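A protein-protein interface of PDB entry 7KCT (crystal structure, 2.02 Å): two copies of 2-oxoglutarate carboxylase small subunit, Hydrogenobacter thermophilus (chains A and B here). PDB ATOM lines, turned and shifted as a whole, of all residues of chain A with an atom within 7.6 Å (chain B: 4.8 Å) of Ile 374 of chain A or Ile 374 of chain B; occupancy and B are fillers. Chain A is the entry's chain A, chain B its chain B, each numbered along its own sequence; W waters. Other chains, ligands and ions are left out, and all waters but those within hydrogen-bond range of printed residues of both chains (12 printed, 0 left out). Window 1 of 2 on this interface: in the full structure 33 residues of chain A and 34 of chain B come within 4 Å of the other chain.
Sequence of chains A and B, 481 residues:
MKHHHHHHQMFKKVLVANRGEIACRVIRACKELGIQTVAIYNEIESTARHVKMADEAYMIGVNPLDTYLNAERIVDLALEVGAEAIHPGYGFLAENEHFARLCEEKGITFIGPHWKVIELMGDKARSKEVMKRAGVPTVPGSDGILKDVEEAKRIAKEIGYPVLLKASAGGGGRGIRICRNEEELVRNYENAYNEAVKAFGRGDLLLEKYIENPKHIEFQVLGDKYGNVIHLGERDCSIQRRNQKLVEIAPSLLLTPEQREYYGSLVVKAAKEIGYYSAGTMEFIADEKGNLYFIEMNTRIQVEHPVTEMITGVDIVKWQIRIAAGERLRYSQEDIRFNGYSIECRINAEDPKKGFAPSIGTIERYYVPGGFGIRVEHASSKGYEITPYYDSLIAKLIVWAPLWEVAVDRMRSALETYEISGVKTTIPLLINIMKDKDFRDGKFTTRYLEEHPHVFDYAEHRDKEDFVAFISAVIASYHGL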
ATOM      1  N   ARG A  28      13.291 -13.328   4.475  1.00  0.00           N
ATOM      2  CA  ARG A  28      11.991 -13.677   5.035  1.00  0.00           C
ATOM      3  C   ARG A  28      11.803 -15.190   5.155  1.00  0.00           C
ATOM      4  O   ARG A  28      11.234 -15.674   6.142  1.00  0.00           O
ATOM      5  CB  ARG A  28      10.854 -13.103   4.177  1.00  0.00           C
ATOM      6  CG  ARG A  28       9.476 -13.525   4.692  1.00  0.00           C
ATOM      7  CD  ARG A  28       8.265 -12.682   4.229  1.00  0.00           C
ATOM      8  NE  ARG A  28       8.525 -11.255   4.319  1.00  0.00           N
ATOM      9  CZ  ARG A  28       8.653 -10.568   5.449  1.00  0.00           C
ATOM     10  NH1 ARG A  28       8.525 -11.177   6.609  1.00  0.00           N
ATOM     11  NH2 ARG A  28       8.939  -9.273   5.414  1.00  0.00           N
ATOM     12  N   GLU A  32      11.197 -17.311   8.730  1.00  0.00           N
ATOM     13  CA  GLU A  32      10.081 -18.227   8.953  1.00  0.00           C
ATOM     14  C   GLU A  32      10.584 -19.618   9.334  1.00  0.00           C
ATOM     15  O   GLU A  32       9.950 -20.300  10.137  1.00  0.00           O
ATOM     16  CB  GLU A  32       9.167 -18.293   7.725  1.00  0.00           C
ATOM     17  CG  GLU A  32       8.350 -16.997   7.485  1.00  0.00           C
ATOM     18  CD  GLU A  32       7.526 -17.018   6.176  1.00  0.00           C
ATOM     19  OE1 GLU A  32       7.596 -18.061   5.485  1.00  0.00           O
ATOM     20  OE2 GLU A  32       6.819 -16.014   5.833  1.00  0.00           O
ATOM     21  N   MET A 310       2.041 -18.604  -6.662  1.00  0.00           N
ATOM     22  CA  MET A 310       0.640 -18.286  -6.394  1.00  0.00           C
ATOM     23  C   MET A 310      -0.329 -19.322  -6.985  1.00  0.00           C
ATOM     24  O   MET A 310      -1.415 -19.498  -6.458  1.00  0.00           O
ATOM     25  CB  MET A 310       0.283 -16.905  -6.932  1.00  0.00           C
ATOM     26  CG  MET A 310       1.267 -15.818  -6.502  1.00  0.00           C
ATOM     27  SD  MET A 310       1.047 -15.413  -4.773  1.00  0.00           S
ATOM     28  CE  MET A 310      -0.305 -14.272  -5.059  1.00  0.00           C
ATOM     29  N   VAL A 368       2.350   1.570  -0.905  1.00  0.00           N
ATOM     30  CA  VAL A 368       2.261   0.201  -1.398  1.00  0.00           C
ATOM     31  C   VAL A 368       0.815  -0.305  -1.348  1.00  0.00           C
ATOM     32  O   VAL A 368       0.217  -0.342  -0.265  1.00  0.00           O
ATOM     33  CB  VAL A 368       3.181  -0.698  -0.550  1.00  0.00           C
ATOM     34  CG1 VAL A 368       3.117  -2.117  -1.008  1.00  0.00           C
ATOM     35  CG2 VAL A 368       4.594  -0.217  -0.624  1.00  0.00           C
ATOM     36  N   PRO A 369       0.238  -0.778  -2.441  1.00  0.00           N
ATOM     37  CA  PRO A 369      -1.126  -1.319  -2.355  1.00  0.00           C
ATOM     38  C   PRO A 369      -1.155  -2.678  -1.666  1.00  0.00           C
ATOM     39  O   PRO A 369      -0.175  -3.415  -1.645  1.00  0.00           O
ATOM     40  CB  PRO A 369      -1.552  -1.426  -3.819  1.00  0.00           C
ATOM     41  CG  PRO A 369      -0.277  -1.768  -4.513  1.00  0.00           C
ATOM     42  CD  PRO A 369       0.805  -0.965  -3.793  1.00  0.00           C
ATOM     43  N   GLY A 370      -2.309  -3.000  -1.089  1.00  0.00           N
ATOM     44  CA  GLY A 370      -2.529  -4.307  -0.498  1.00  0.00           C
ATOM     45  C   GLY A 370      -3.988  -4.698  -0.649  1.00  0.00           C
ATOM     46  O   GLY A 370      -4.862  -3.853  -0.853  1.00  0.00           O
ATOM     47  N   GLY A 371      -4.236  -6.002  -0.597  1.00  0.00           N
ATOM     48  CA  GLY A 371      -5.592  -6.493  -0.580  1.00  0.00           C
ATOM     49  C   GLY A 371      -5.675  -7.979  -0.891  1.00  0.00           C
ATOM     50  O   GLY A 371      -4.670  -8.705  -0.973  1.00  0.00           O
ATOM     51  N   PHE A 372      -6.925  -8.404  -1.062  1.00  0.00           N
ATOM     52  CA  PHE A 372      -7.233  -9.776  -1.434  1.00  0.00           C
ATOM     53  C   PHE A 372      -6.555 -10.065  -2.769  1.00  0.00           C
ATOM     54  O   PHE A 372      -6.719  -9.314  -3.737  1.00  0.00           O
ATOM     55  CB  PHE A 372      -8.765  -9.909  -1.511  1.00  0.00           C
ATOM     56  CG  PHE A 372      -9.270 -11.281  -1.907  1.00  0.00           C
ATOM     57  CD1 PHE A 372      -9.147 -11.749  -3.218  1.00  0.00           C
ATOM     58  CD2 PHE A 372      -9.894 -12.083  -0.978  1.00  0.00           C
ATOM     59  CE1 PHE A 372      -9.611 -13.028  -3.571  1.00  0.00           C
ATOM     60  CE2 PHE A 372     -10.371 -13.361  -1.321  1.00  0.00           C
ATOM     61  CZ  PHE A 372     -10.231 -13.829  -2.611  1.00  0.00           C
ATOM     62  N   GLY A 373      -5.743 -11.116  -2.800  1.00  0.00           N
ATOM     63  CA  GLY A 373      -5.063 -11.517  -4.016  1.00  0.00           C
ATOM     64  C   GLY A 373      -3.903 -10.648  -4.465  1.00  0.00           C
ATOM     65  O   GLY A 373      -3.442 -10.799  -5.596  1.00  0.00           O
ATOM     66  N   ILE A 374      -3.368  -9.790  -3.599  1.00  0.00           N
ATOM     67  CA  ILE A 374      -2.245  -8.927  -3.943  1.00  0.00           C
ATOM     68  C   ILE A 374      -1.025  -9.295  -3.087  1.00  0.00           C
ATOM     69  O   ILE A 374      -1.125  -9.427  -1.857  1.00  0.00           O
ATOM     70  CB  ILE A 374      -2.657  -7.457  -3.779  1.00  0.00           C
ATOM     71  CG1 ILE A 374      -3.716  -7.017  -4.808  1.00  0.00           C
ATOM     72  CG2 ILE A 374      -1.458  -6.552  -3.880  1.00  0.00           C
ATOM     73  CD1 ILE A 374      -4.332  -5.628  -4.487  1.00  0.00           C
ATOM     74  N   ARG A 375       0.121  -9.431  -3.732  1.00  0.00           N
ATOM     75  CA  ARG A 375       1.393  -9.639  -3.051  1.00  0.00           C
ATOM     76  C   ARG A 375       2.366  -8.612  -3.588  1.00  0.00           C
ATOM     77  O   ARG A 375       2.393  -8.324  -4.790  1.00  0.00           O
ATOM     78  CB  ARG A 375       1.888 -11.092  -3.278  1.00  0.00           C
ATOM     79  CG  ARG A 375       3.301 -11.424  -2.898  1.00  0.00           C
ATOM     80  CD  ARG A 375       3.573 -12.890  -3.206  1.00  0.00           C
ATOM     81  NE  ARG A 375       4.963 -13.239  -3.023  1.00  0.00           N
ATOM     82  CZ  ARG A 375       5.455 -14.448  -3.223  1.00  0.00           C
ATOM     83  NH1 ARG A 375       4.668 -15.456  -3.634  1.00  0.00           N
ATOM     84  NH2 ARG A 375       6.729 -14.635  -3.018  1.00  0.00           N
ATOM     85  N   VAL A 376       3.184  -8.071  -2.706  1.00  0.00           N
ATOM     86  CA  VAL A 376       4.172  -7.085  -3.088  1.00  0.00           C
ATOM     87  C   VAL A 376       5.524  -7.576  -2.619  1.00  0.00           C
ATOM     88  O   VAL A 376       5.674  -7.932  -1.442  1.00  0.00           O
ATOM     89  CB  VAL A 376       3.888  -5.697  -2.495  1.00  0.00           C
ATOM     90  CG1 VAL A 376       4.982  -4.707  -2.977  1.00  0.00           C
ATOM     91  CG2 VAL A 376       2.534  -5.217  -2.924  1.00  0.00           C
ATOM     92  N   GLU A 377       6.500  -7.592  -3.528  1.00  0.00           N
ATOM     93  CA  GLU A 377       7.901  -7.877  -3.218  1.00  0.00           C
ATOM     94  C   GLU A 377       8.688  -6.580  -3.418  1.00  0.00           C
ATOM     95  O   GLU A 377       8.798  -6.073  -4.539  1.00  0.00           O
ATOM     96  CB  GLU A 377       8.454  -9.001  -4.093  1.00  0.00           C
ATOM     97  CG  GLU A 377       7.698 -10.320  -3.950  1.00  0.00           C
ATOM     98  CD  GLU A 377       8.120 -11.177  -2.726  1.00  0.00           C
ATOM     99  OE1 GLU A 377       9.249 -11.011  -2.138  1.00  0.00           O
ATOM    100  OE2 GLU A 377       7.290 -12.042  -2.359  1.00  0.00           O
ATOM    101  N   LEU A 397       5.023  -6.323  -8.319  1.00  0.00           N
ATOM    102  CA  LEU A 397       3.628  -6.407  -7.930  1.00  0.00           C
ATOM    103  C   LEU A 397       3.058  -7.701  -8.496  1.00  0.00           C
ATOM    104  O   LEU A 397       3.126  -7.920  -9.703  1.00  0.00           O
ATOM    105  CB  LEU A 397       2.860  -5.203  -8.449  1.00  0.00           C
ATOM    106  CG  LEU A 397       1.403  -5.066  -8.090  1.00  0.00           C
ATOM    107  CD1 LEU A 397       1.317  -5.090  -6.607  1.00  0.00           C
ATOM    108  CD2 LEU A 397       0.942  -3.735  -8.734  1.00  0.00           C
ATOM    109  N   ILE A 398       2.503  -8.554  -7.638  1.00  0.00           N
ATOM    110  CA  ILE A 398       1.997  -9.865  -8.051  1.00  0.00           C
ATOM    111  C   ILE A 398       0.549  -9.975  -7.663  1.00  0.00           C
ATOM    112  O   ILE A 398       0.190  -9.621  -6.534  1.00  0.00           O
ATOM    113  CB  ILE A 398       2.790 -11.012  -7.410  1.00  0.00           C
ATOM    114  CG1 ILE A 398       4.254 -10.871  -7.768  1.00  0.00           C
ATOM    115  CG2 ILE A 398       2.214 -12.387  -7.853  1.00  0.00           C
ATOM    116  CD1 ILE A 398       5.135 -10.639  -6.578  1.00  0.00           C
ATOM    117  N   VAL A 399      -0.299 -10.457  -8.581  1.00  0.00           N
ATOM    118  CA  VAL A 399      -1.691 -10.668  -8.240  1.00  0.00           C
ATOM    119  C   VAL A 399      -2.097 -12.082  -8.607  1.00  0.00           C
ATOM    120  O   VAL A 399      -1.434 -12.770  -9.390  1.00  0.00           O
ATOM    121  CB  VAL A 399      -2.690  -9.663  -8.881  1.00  0.00           C
ATOM    122  CG1 VAL A 399      -2.238  -8.240  -8.613  1.00  0.00           C
ATOM    123  CG2 VAL A 399      -2.933  -9.923 -10.410  1.00  0.00           C
ATOM    124  N   TRP A 400      -3.187 -12.515  -7.989  1.00  0.00           N
ATOM    125  CA  TRP A 400      -3.776 -13.827  -8.255  1.00  0.00           C
ATOM    126  C   TRP A 400      -5.289 -13.673  -8.356  1.00  0.00           C
ATOM    127  O   TRP A 400      -5.879 -12.875  -7.626  1.00  0.00           O
ATOM    128  CB  TRP A 400      -3.432 -14.878  -7.145  1.00  0.00           C
ATOM    129  CG  TRP A 400      -4.145 -16.235  -7.400  1.00  0.00           C
ATOM    130  CD1 TRP A 400      -3.658 -17.290  -8.101  1.00  0.00           C
ATOM    131  CD2 TRP A 400      -5.450 -16.619  -6.967  1.00  0.00           C
ATOM    132  NE1 TRP A 400      -4.584 -18.326  -8.131  1.00  0.00           N
ATOM    133  CE2 TRP A 400      -5.701 -17.918  -7.453  1.00  0.00           C
ATOM    134  CE3 TRP A 400      -6.425 -15.998  -6.192  1.00  0.00           C
ATOM    135  CZ2 TRP A 400      -6.901 -18.579  -7.219  1.00  0.00           C
ATOM    136  CZ3 TRP A 400      -7.597 -16.644  -5.969  1.00  0.00           C
ATOM    137  CH2 TRP A 400      -7.827 -17.930  -6.474  1.00  0.00           C
ATOM    138  N   ARG A 410      -7.614  -6.995 -11.467  1.00  0.00           N
ATOM    139  CA  ARG A 410      -6.990  -6.841 -10.163  1.00  0.00           C
ATOM    140  C   ARG A 410      -5.627  -6.174 -10.284  1.00  0.00           C
ATOM    141  O   ARG A 410      -5.269  -5.335  -9.453  1.00  0.00           O
ATOM    142  CB  ARG A 410      -6.864  -8.210  -9.487  1.00  0.00           C
ATOM    143  CG  ARG A 410      -6.119  -8.200  -8.160  1.00  0.00           C
ATOM    144  CD  ARG A 410      -6.516  -9.493  -7.413  1.00  0.00           C
ATOM    145  NE  ARG A 410      -7.889  -9.334  -6.948  1.00  0.00           N
ATOM    146  CZ  ARG A 410      -8.743 -10.315  -6.684  1.00  0.00           C
ATOM    147  NH1 ARG A 410      -8.411 -11.582  -6.887  1.00  0.00           N
ATOM    148  NH2 ARG A 410      -9.952 -10.011  -6.251  1.00  0.00           N
ATOM    149  N   MET A 411      -4.849  -6.518 -11.319  1.00  0.00           N
ATOM    150  CA  MET A 411      -3.539  -5.893 -11.507  1.00  0.00           C
ATOM    151  C   MET A 411      -3.661  -4.429 -11.942  1.00  0.00           C
ATOM    152  O   MET A 411      -2.912  -3.566 -11.460  1.00  0.00           O
ATOM    153  CB  MET A 411      -2.719  -6.688 -12.544  1.00  0.00           C
ATOM    154  CG  MET A 411      -1.395  -6.046 -12.903  1.00  0.00           C
ATOM    155  SD  MET A 411      -0.156  -5.979 -11.562  1.00  0.00           S
ATOM    156  CE  MET A 411       0.378  -7.672 -11.527  1.00  0.00           C
ATOM    157  N   SER A 413      -5.977  -2.400 -11.168  1.00  0.00           N
ATOM    158  CA  SER A 413      -6.424  -1.647  -9.998  1.00  0.00           C
ATOM    159  C   SER A 413      -5.331  -1.489  -8.950  1.00  0.00           C
ATOM    160  O   SER A 413      -5.295  -0.484  -8.234  1.00  0.00           O
ATOM    161  CB  SER A 413      -7.630  -2.332  -9.355  1.00  0.00           C
ATOM    162  OG  SER A 413      -8.719  -2.304 -10.232  1.00  0.00           O
ATOM    163  N   ALA A 414      -4.515  -2.519  -8.767  1.00  0.00           N
ATOM    164  CA  ALA A 414      -3.374  -2.421  -7.872  1.00  0.00           C
ATOM    165  C   ALA A 414      -2.388  -1.381  -8.389  1.00  0.00           C
ATOM    166  O   ALA A 414      -1.975  -0.480  -7.648  1.00  0.00           O
ATOM    167  CB  ALA A 414      -2.707  -3.791  -7.726  1.00  0.00           C
ATOM    168  N   LEU A 415      -2.088  -1.427  -9.686  1.00  0.00           N
ATOM    169  CA  LEU A 415      -1.138  -0.487 -10.285  1.00  0.00           C
ATOM    170  C   LEU A 415      -1.619   0.963 -10.186  1.00  0.00           C
ATOM    171  O   LEU A 415      -0.824   1.897  -9.964  1.00  0.00           O
ATOM    172  CB  LEU A 415      -0.944  -0.858 -11.751  1.00  0.00           C
ATOM    173  CG  LEU A 415      -0.129  -2.073 -12.152  1.00  0.00           C
ATOM    174  CD1 LEU A 415      -0.369  -2.421 -13.614  1.00  0.00           C
ATOM    175  CD2 LEU A 415       1.356  -1.803 -11.877  1.00  0.00           C
ATOM    176  N   THR A 417      -3.200   2.261  -7.916  1.00  0.00           N
ATOM    177  CA  THR A 417      -3.087   2.779  -6.553  1.00  0.00           C
ATOM    178  C   THR A 417      -1.664   2.762  -5.999  1.00  0.00           C
ATOM    179  O   THR A 417      -1.443   3.243  -4.891  1.00  0.00           O
ATOM    180  CB  THR A 417      -4.017   2.011  -5.612  1.00  0.00           C
ATOM    181  OG1 THR A 417      -3.554   0.673  -5.432  1.00  0.00           O
ATOM    182  CG2 THR A 417      -5.419   1.994  -6.152  1.00  0.00           C
ATOM    183  N   ARG B  28     -10.988  -0.434  -3.631  1.00  0.00           N
ATOM    184  CA  ARG B  28     -10.307  -1.440  -4.440  1.00  0.00           C
ATOM    185  C   ARG B  28     -11.297  -2.431  -5.066  1.00  0.00           C
ATOM    186  O   ARG B  28     -11.203  -2.759  -6.255  1.00  0.00           O
ATOM    187  CB  ARG B  28      -9.264  -2.200  -3.604  1.00  0.00           C
ATOM    188  CG  ARG B  28      -8.593  -3.366  -4.395  1.00  0.00           C
ATOM    189  CD  ARG B  28      -7.290  -3.933  -3.839  1.00  0.00           C
ATOM    190  NE  ARG B  28      -6.418  -2.851  -3.436  1.00  0.00           N
ATOM    191  CZ  ARG B  28      -5.838  -1.989  -4.260  1.00  0.00           C
ATOM    192  NH1 ARG B  28      -5.994  -2.095  -5.590  1.00  0.00           N
ATOM    193  NH2 ARG B  28      -5.123  -1.010  -3.747  1.00  0.00           N
ATOM    194  N   PRO B 369       5.839  -4.855   5.120  1.00  0.00           N
ATOM    195  CA  PRO B 369       6.307  -6.161   4.620  1.00  0.00           C
ATOM    196  C   PRO B 369       5.431  -6.760   3.531  1.00  0.00           C
ATOM    197  O   PRO B 369       4.237  -6.485   3.399  1.00  0.00           O
ATOM    198  CB  PRO B 369       6.275  -7.056   5.870  1.00  0.00           C
ATOM    199  CG  PRO B 369       5.275  -6.446   6.751  1.00  0.00           C
ATOM    200  CD  PRO B 369       5.284  -4.965   6.480  1.00  0.00           C
ATOM    201  N   GLY B 370       6.052  -7.623   2.750  1.00  0.00           N
ATOM    202  CA  GLY B 370       5.309  -8.395   1.781  1.00  0.00           C
ATOM    203  C   GLY B 370       5.981  -9.729   1.584  1.00  0.00           C
ATOM    204  O   GLY B 370       7.157  -9.916   1.908  1.00  0.00           O
ATOM    205  N   GLY B 371       5.227 -10.655   1.017  1.00  0.00           N
ATOM    206  CA  GLY B 371       5.767 -11.969   0.772  1.00  0.00           C
ATOM    207  C   GLY B 371       4.674 -12.989   0.544  1.00  0.00           C
ATOM    208  O   GLY B 371       3.479 -12.692   0.557  1.00  0.00           O
ATOM    209  N   PHE B 372       5.136 -14.202   0.306  1.00  0.00           N
ATOM    210  CA  PHE B 372       4.233 -15.342   0.184  1.00  0.00           C
ATOM    211  C   PHE B 372       3.370 -15.451   1.419  1.00  0.00           C
ATOM    212  O   PHE B 372       3.882 -15.535   2.544  1.00  0.00           O
ATOM    213  CB  PHE B 372       5.031 -16.597   0.055  1.00  0.00           C
ATOM    214  CG  PHE B 372       4.234 -17.845  -0.299  1.00  0.00           C
ATOM    215  CD1 PHE B 372       3.757 -18.064  -1.584  1.00  0.00           C
ATOM    216  CD2 PHE B 372       4.058 -18.846   0.639  1.00  0.00           C
ATOM    217  CE1 PHE B 372       3.118 -19.292  -1.917  1.00  0.00           C
ATOM    218  CE2 PHE B 372       3.433 -20.055   0.305  1.00  0.00           C
ATOM    219  CZ  PHE B 372       2.985 -20.276  -0.968  1.00  0.00           C
ATOM    220  N   GLY B 373       2.068 -15.472   1.198  1.00  0.00           N
ATOM    221  CA  GLY B 373       1.120 -15.626   2.272  1.00  0.00           C
ATOM    222  C   GLY B 373       0.914 -14.395   3.150  1.00  0.00           C
ATOM    223  O   GLY B 373       0.379 -14.525   4.238  1.00  0.00           O
ATOM    224  N   ILE B 374       1.291 -13.207   2.705  1.00  0.00           N
ATOM    225  CA  ILE B 374       1.125 -11.996   3.500  1.00  0.00           C
ATOM    226  C   ILE B 374       0.218 -11.023   2.760  1.00  0.00           C
ATOM    227  O   ILE B 374       0.365 -10.792   1.546  1.00  0.00           O
ATOM    228  CB  ILE B 374       2.472 -11.338   3.824  1.00  0.00           C
ATOM    229  CG1 ILE B 374       3.270 -12.170   4.795  1.00  0.00           C
ATOM    230  CG2 ILE B 374       2.279  -9.990   4.483  1.00  0.00           C
ATOM    231  CD1 ILE B 374       4.736 -11.852   4.721  1.00  0.00           C
ATOM    232  N   ARG B 375      -0.718 -10.451   3.499  1.00  0.00           N
ATOM    233  CA  ARG B 375      -1.602  -9.414   3.000  1.00  0.00           C
ATOM    234  C   ARG B 375      -1.588  -8.277   3.993  1.00  0.00           C
ATOM    235  O   ARG B 375      -1.612  -8.488   5.210  1.00  0.00           O
ATOM    236  CB  ARG B 375      -3.026  -9.954   2.836  1.00  0.00           C
ATOM    237  CG  ARG B 375      -4.128  -8.993   2.439  1.00  0.00           C
ATOM    238  CD  ARG B 375      -5.467  -9.760   2.494  1.00  0.00           C
ATOM    239  NE  ARG B 375      -6.641  -8.903   2.360  1.00  0.00           N
ATOM    240  CZ  ARG B 375      -7.894  -9.363   2.281  1.00  0.00           C
ATOM    241  NH1 ARG B 375      -8.127 -10.686   2.368  1.00  0.00           N
ATOM    242  NH2 ARG B 375      -8.900  -8.501   2.096  1.00  0.00           N
ATOM    243  N   VAL B 376      -1.592  -7.068   3.482  1.00  0.00           N
ATOM    244  CA  VAL B 376      -1.609  -5.891   4.330  1.00  0.00           C
ATOM    245  C   VAL B 376      -2.778  -5.011   3.931  1.00  0.00           C
ATOM    246  O   VAL B 376      -3.013  -4.774   2.737  1.00  0.00           O
ATOM    247  CB  VAL B 376      -0.290  -5.122   4.230  1.00  0.00           C
ATOM    248  CG1 VAL B 376      -0.290  -3.953   5.236  1.00  0.00           C
ATOM    249  CG2 VAL B 376       0.866  -6.049   4.493  1.00  0.00           C
ATOM    250  N   LEU B 397      -2.221  -6.408   9.470  1.00  0.00           N
ATOM    251  CA  LEU B 397      -1.307  -7.382   8.911  1.00  0.00           C
ATOM    252  C   LEU B 397      -1.997  -8.733   8.955  1.00  0.00           C
ATOM    253  O   LEU B 397      -2.391  -9.178  10.037  1.00  0.00           O
ATOM    254  CB  LEU B 397      -0.053  -7.417   9.768  1.00  0.00           C
ATOM    255  CG  LEU B 397       1.056  -8.321   9.319  1.00  0.00           C
ATOM    256  CD1 LEU B 397       1.352  -8.094   7.935  1.00  0.00           C
ATOM    257  CD2 LEU B 397       2.257  -8.127  10.172  1.00  0.00           C
ATOM    258  N   ILE B 398      -2.097  -9.408   7.811  1.00  0.00           N
ATOM    259  CA  ILE B 398      -2.803 -10.680   7.714  1.00  0.00           C
ATOM    260  C   ILE B 398      -1.885 -11.707   7.077  1.00  0.00           C
ATOM    261  O   ILE B 398      -1.198 -11.400   6.101  1.00  0.00           O
ATOM    262  CB  ILE B 398      -4.116 -10.554   6.900  1.00  0.00           C
ATOM    263  CG1 ILE B 398      -5.054  -9.490   7.463  1.00  0.00           C
ATOM    264  CG2 ILE B 398      -4.806 -11.890   6.829  1.00  0.00           C
ATOM    265  CD1 ILE B 398      -5.374  -8.382   6.426  1.00  0.00           C
ATOM    266  N   VAL B 399      -1.856 -12.928   7.626  1.00  0.00           N
ATOM    267  CA  VAL B 399      -1.044 -13.990   7.053  1.00  0.00           C
ATOM    268  C   VAL B 399      -1.902 -15.237   6.896  1.00  0.00           C
ATOM    269  O   VAL B 399      -2.924 -15.392   7.553  1.00  0.00           O
ATOM    270  CB  VAL B 399       0.217 -14.314   7.890  1.00  0.00           C
ATOM    271  CG1 VAL B 399       1.015 -13.016   8.196  1.00  0.00           C
ATOM    272  CG2 VAL B 399      -0.155 -15.079   9.137  1.00  0.00           C
ATOM    273  N   ARG B 410       5.066 -17.242  10.313  1.00  0.00           N
ATOM    274  CA  ARG B 410       4.885 -16.231   9.276  1.00  0.00           C
ATOM    275  C   ARG B 410       4.462 -14.886   9.861  1.00  0.00           C
ATOM    276  O   ARG B 410       5.009 -13.850   9.483  1.00  0.00           O
ATOM    277  CB  ARG B 410       3.869 -16.701   8.254  1.00  0.00           C
ATOM    278  CG  ARG B 410       3.594 -15.728   7.107  1.00  0.00           C
ATOM    279  CD  ARG B 410       3.008 -16.501   5.882  1.00  0.00           C
ATOM    280  NE  ARG B 410       4.091 -17.260   5.268  1.00  0.00           N
ATOM    281  CZ  ARG B 410       3.962 -18.371   4.555  1.00  0.00           C
ATOM    282  NH1 ARG B 410       2.767 -18.896   4.297  1.00  0.00           N
ATOM    283  NH2 ARG B 410       5.050 -18.933   4.075  1.00  0.00           N
ATOM    284  N   ALA B 414       6.729 -11.463   9.798  1.00  0.00           N
ATOM    285  CA  ALA B 414       6.191 -10.264   9.149  1.00  0.00           C
ATOM    286  C   ALA B 414       6.200  -9.080  10.101  1.00  0.00           C
ATOM    287  O   ALA B 414       6.684  -8.000   9.740  1.00  0.00           O
ATOM    288  CB  ALA B 414       4.774 -10.495   8.627  1.00  0.00           C
HETATM  289  O   HOH W   1       6.527 -15.505   3.157  1.00  0.00           O
HETATM  290  O   HOH W   2      -4.363  -0.762  -0.887  1.00  0.00           O
HETATM  291  O   HOH W   3      -1.686  -7.395   0.139  1.00  0.00           O
HETATM  292  O   HOH W   4       2.619  -9.363   0.196  1.00  0.00           O
HETATM  293  O   HOH W   5       6.949 -13.577   7.159  1.00  0.00           O
HETATM  294  O   HOH W   6      -1.057 -11.673  -0.598  1.00  0.00           O
HETATM  295  O   HOH W   7      -3.815  -2.118   1.826  1.00  0.00           O
HETATM  296  O   HOH W   8       0.860 -14.797  -1.263  1.00  0.00           O
HETATM  297  O   HOH W   9      -6.596  -4.502  -7.138  1.00  0.00           O
HETATM  298  O   HOH W  10       9.247  -7.841   2.865  1.00  0.00           O
HETATM  299  O   HOH W  11       8.328  -7.514   0.127  1.00  0.00           O
HETATM  300  O   HOH W  12       9.291 -11.777   0.551  1.00  0.00           O
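Ile 374 of chain A touches just these residues of chain B: Arg 28 (3.5 Å) and Ile 374 (3.96 Å). Ile 374 of chain B touches two residues of chain A. No residue of chain A comes within 4 Å of Gly 373 of chain B. Of the printed residues of chain B, Phe 372 of chain A touches Arg 375. Of the printed residues of chain A, Arg 410 of chain B touches Glu 32 (3.0 Å). Leu 415 of chain A touches none of the printed residues of chain B. The nearest printed residue of chain B that does not touch Ile 374 of chain A is Arg 375 of chain B (4.9 Å). The nearest printed residue of chain A that does not touch Gly 371 of chain B is Arg 28 of chain A (4.3 Å).
The guanidinium group of Arg 28 of chain A sits at hydrogen-bond distance from the backbone carbonyl oxygen of Gly 370 of chain B. The side-chain carboxylate of Glu 32 of chain A lies within salt-bridge range of the guanidinium group of Arg 410 of chain B, 3.0 Å away. O of Gly 370 of chain A sits at hydrogen-bond distance from NE of Arg 28 of chain B, 3.2 Å away. O of Ser 413 of chain A sits at hydrogen-bond distance from NH1 of Arg 28 of chain B, 3.2 Å away. NH2 of Arg 28 of chain B is in hydrogen-bond range of OG1 of Thr 417 of chain A, at 2.9 Å. The backbone NH (N) of Phe 372 of chain A sits close to the guanidinium group (NE) of Arg 375 of chain B (3.5 Å). The guanidinium group (NE) of Arg 375 of chain A sits close to the backbone NH (N) of Phe 372 of chain B (3.5 Å).
Gly 371 of chain A touches Arg 375 of chain B, and with the chains exchanged Arg 375 of chain A touches Gly 371 of chain B. Positions printed for both chains: 28, 369, 370, 371, 372, 373, 374, 375, 376, 397, 398, 399, 410 and 414.
Water W8 lies within hydrogen-bond range of N of Gly 373 of chain B (2.8 Å) and SD of Met 310 of chain A (3.6 Å).
The guanidinium group (NE) of Arg 375 of chain A is in salt-bridge range of the side-chain carboxylate (OE2) of Glu 377 of chain A, 2.7 Å away.
Of the 14 printed residues of chain B, 10 touch a printed residue of chain A. Of the 23 printed residues of chain A, 13 touch a printed residue of chain B. Hydrophobic or aromatic side chains of chain A that line the printed part of chain B: Pro 369, Phe 372 and Ile 374. Among the printed residues, 21 pairs touch across the chains. Among the printed residues, Asp or Glu carboxylates within 4 Å of a Lys or Arg side-chain nitrogen of the other chain: Glu 32 of chain A with Arg 410 of chain B (3.0 Å).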
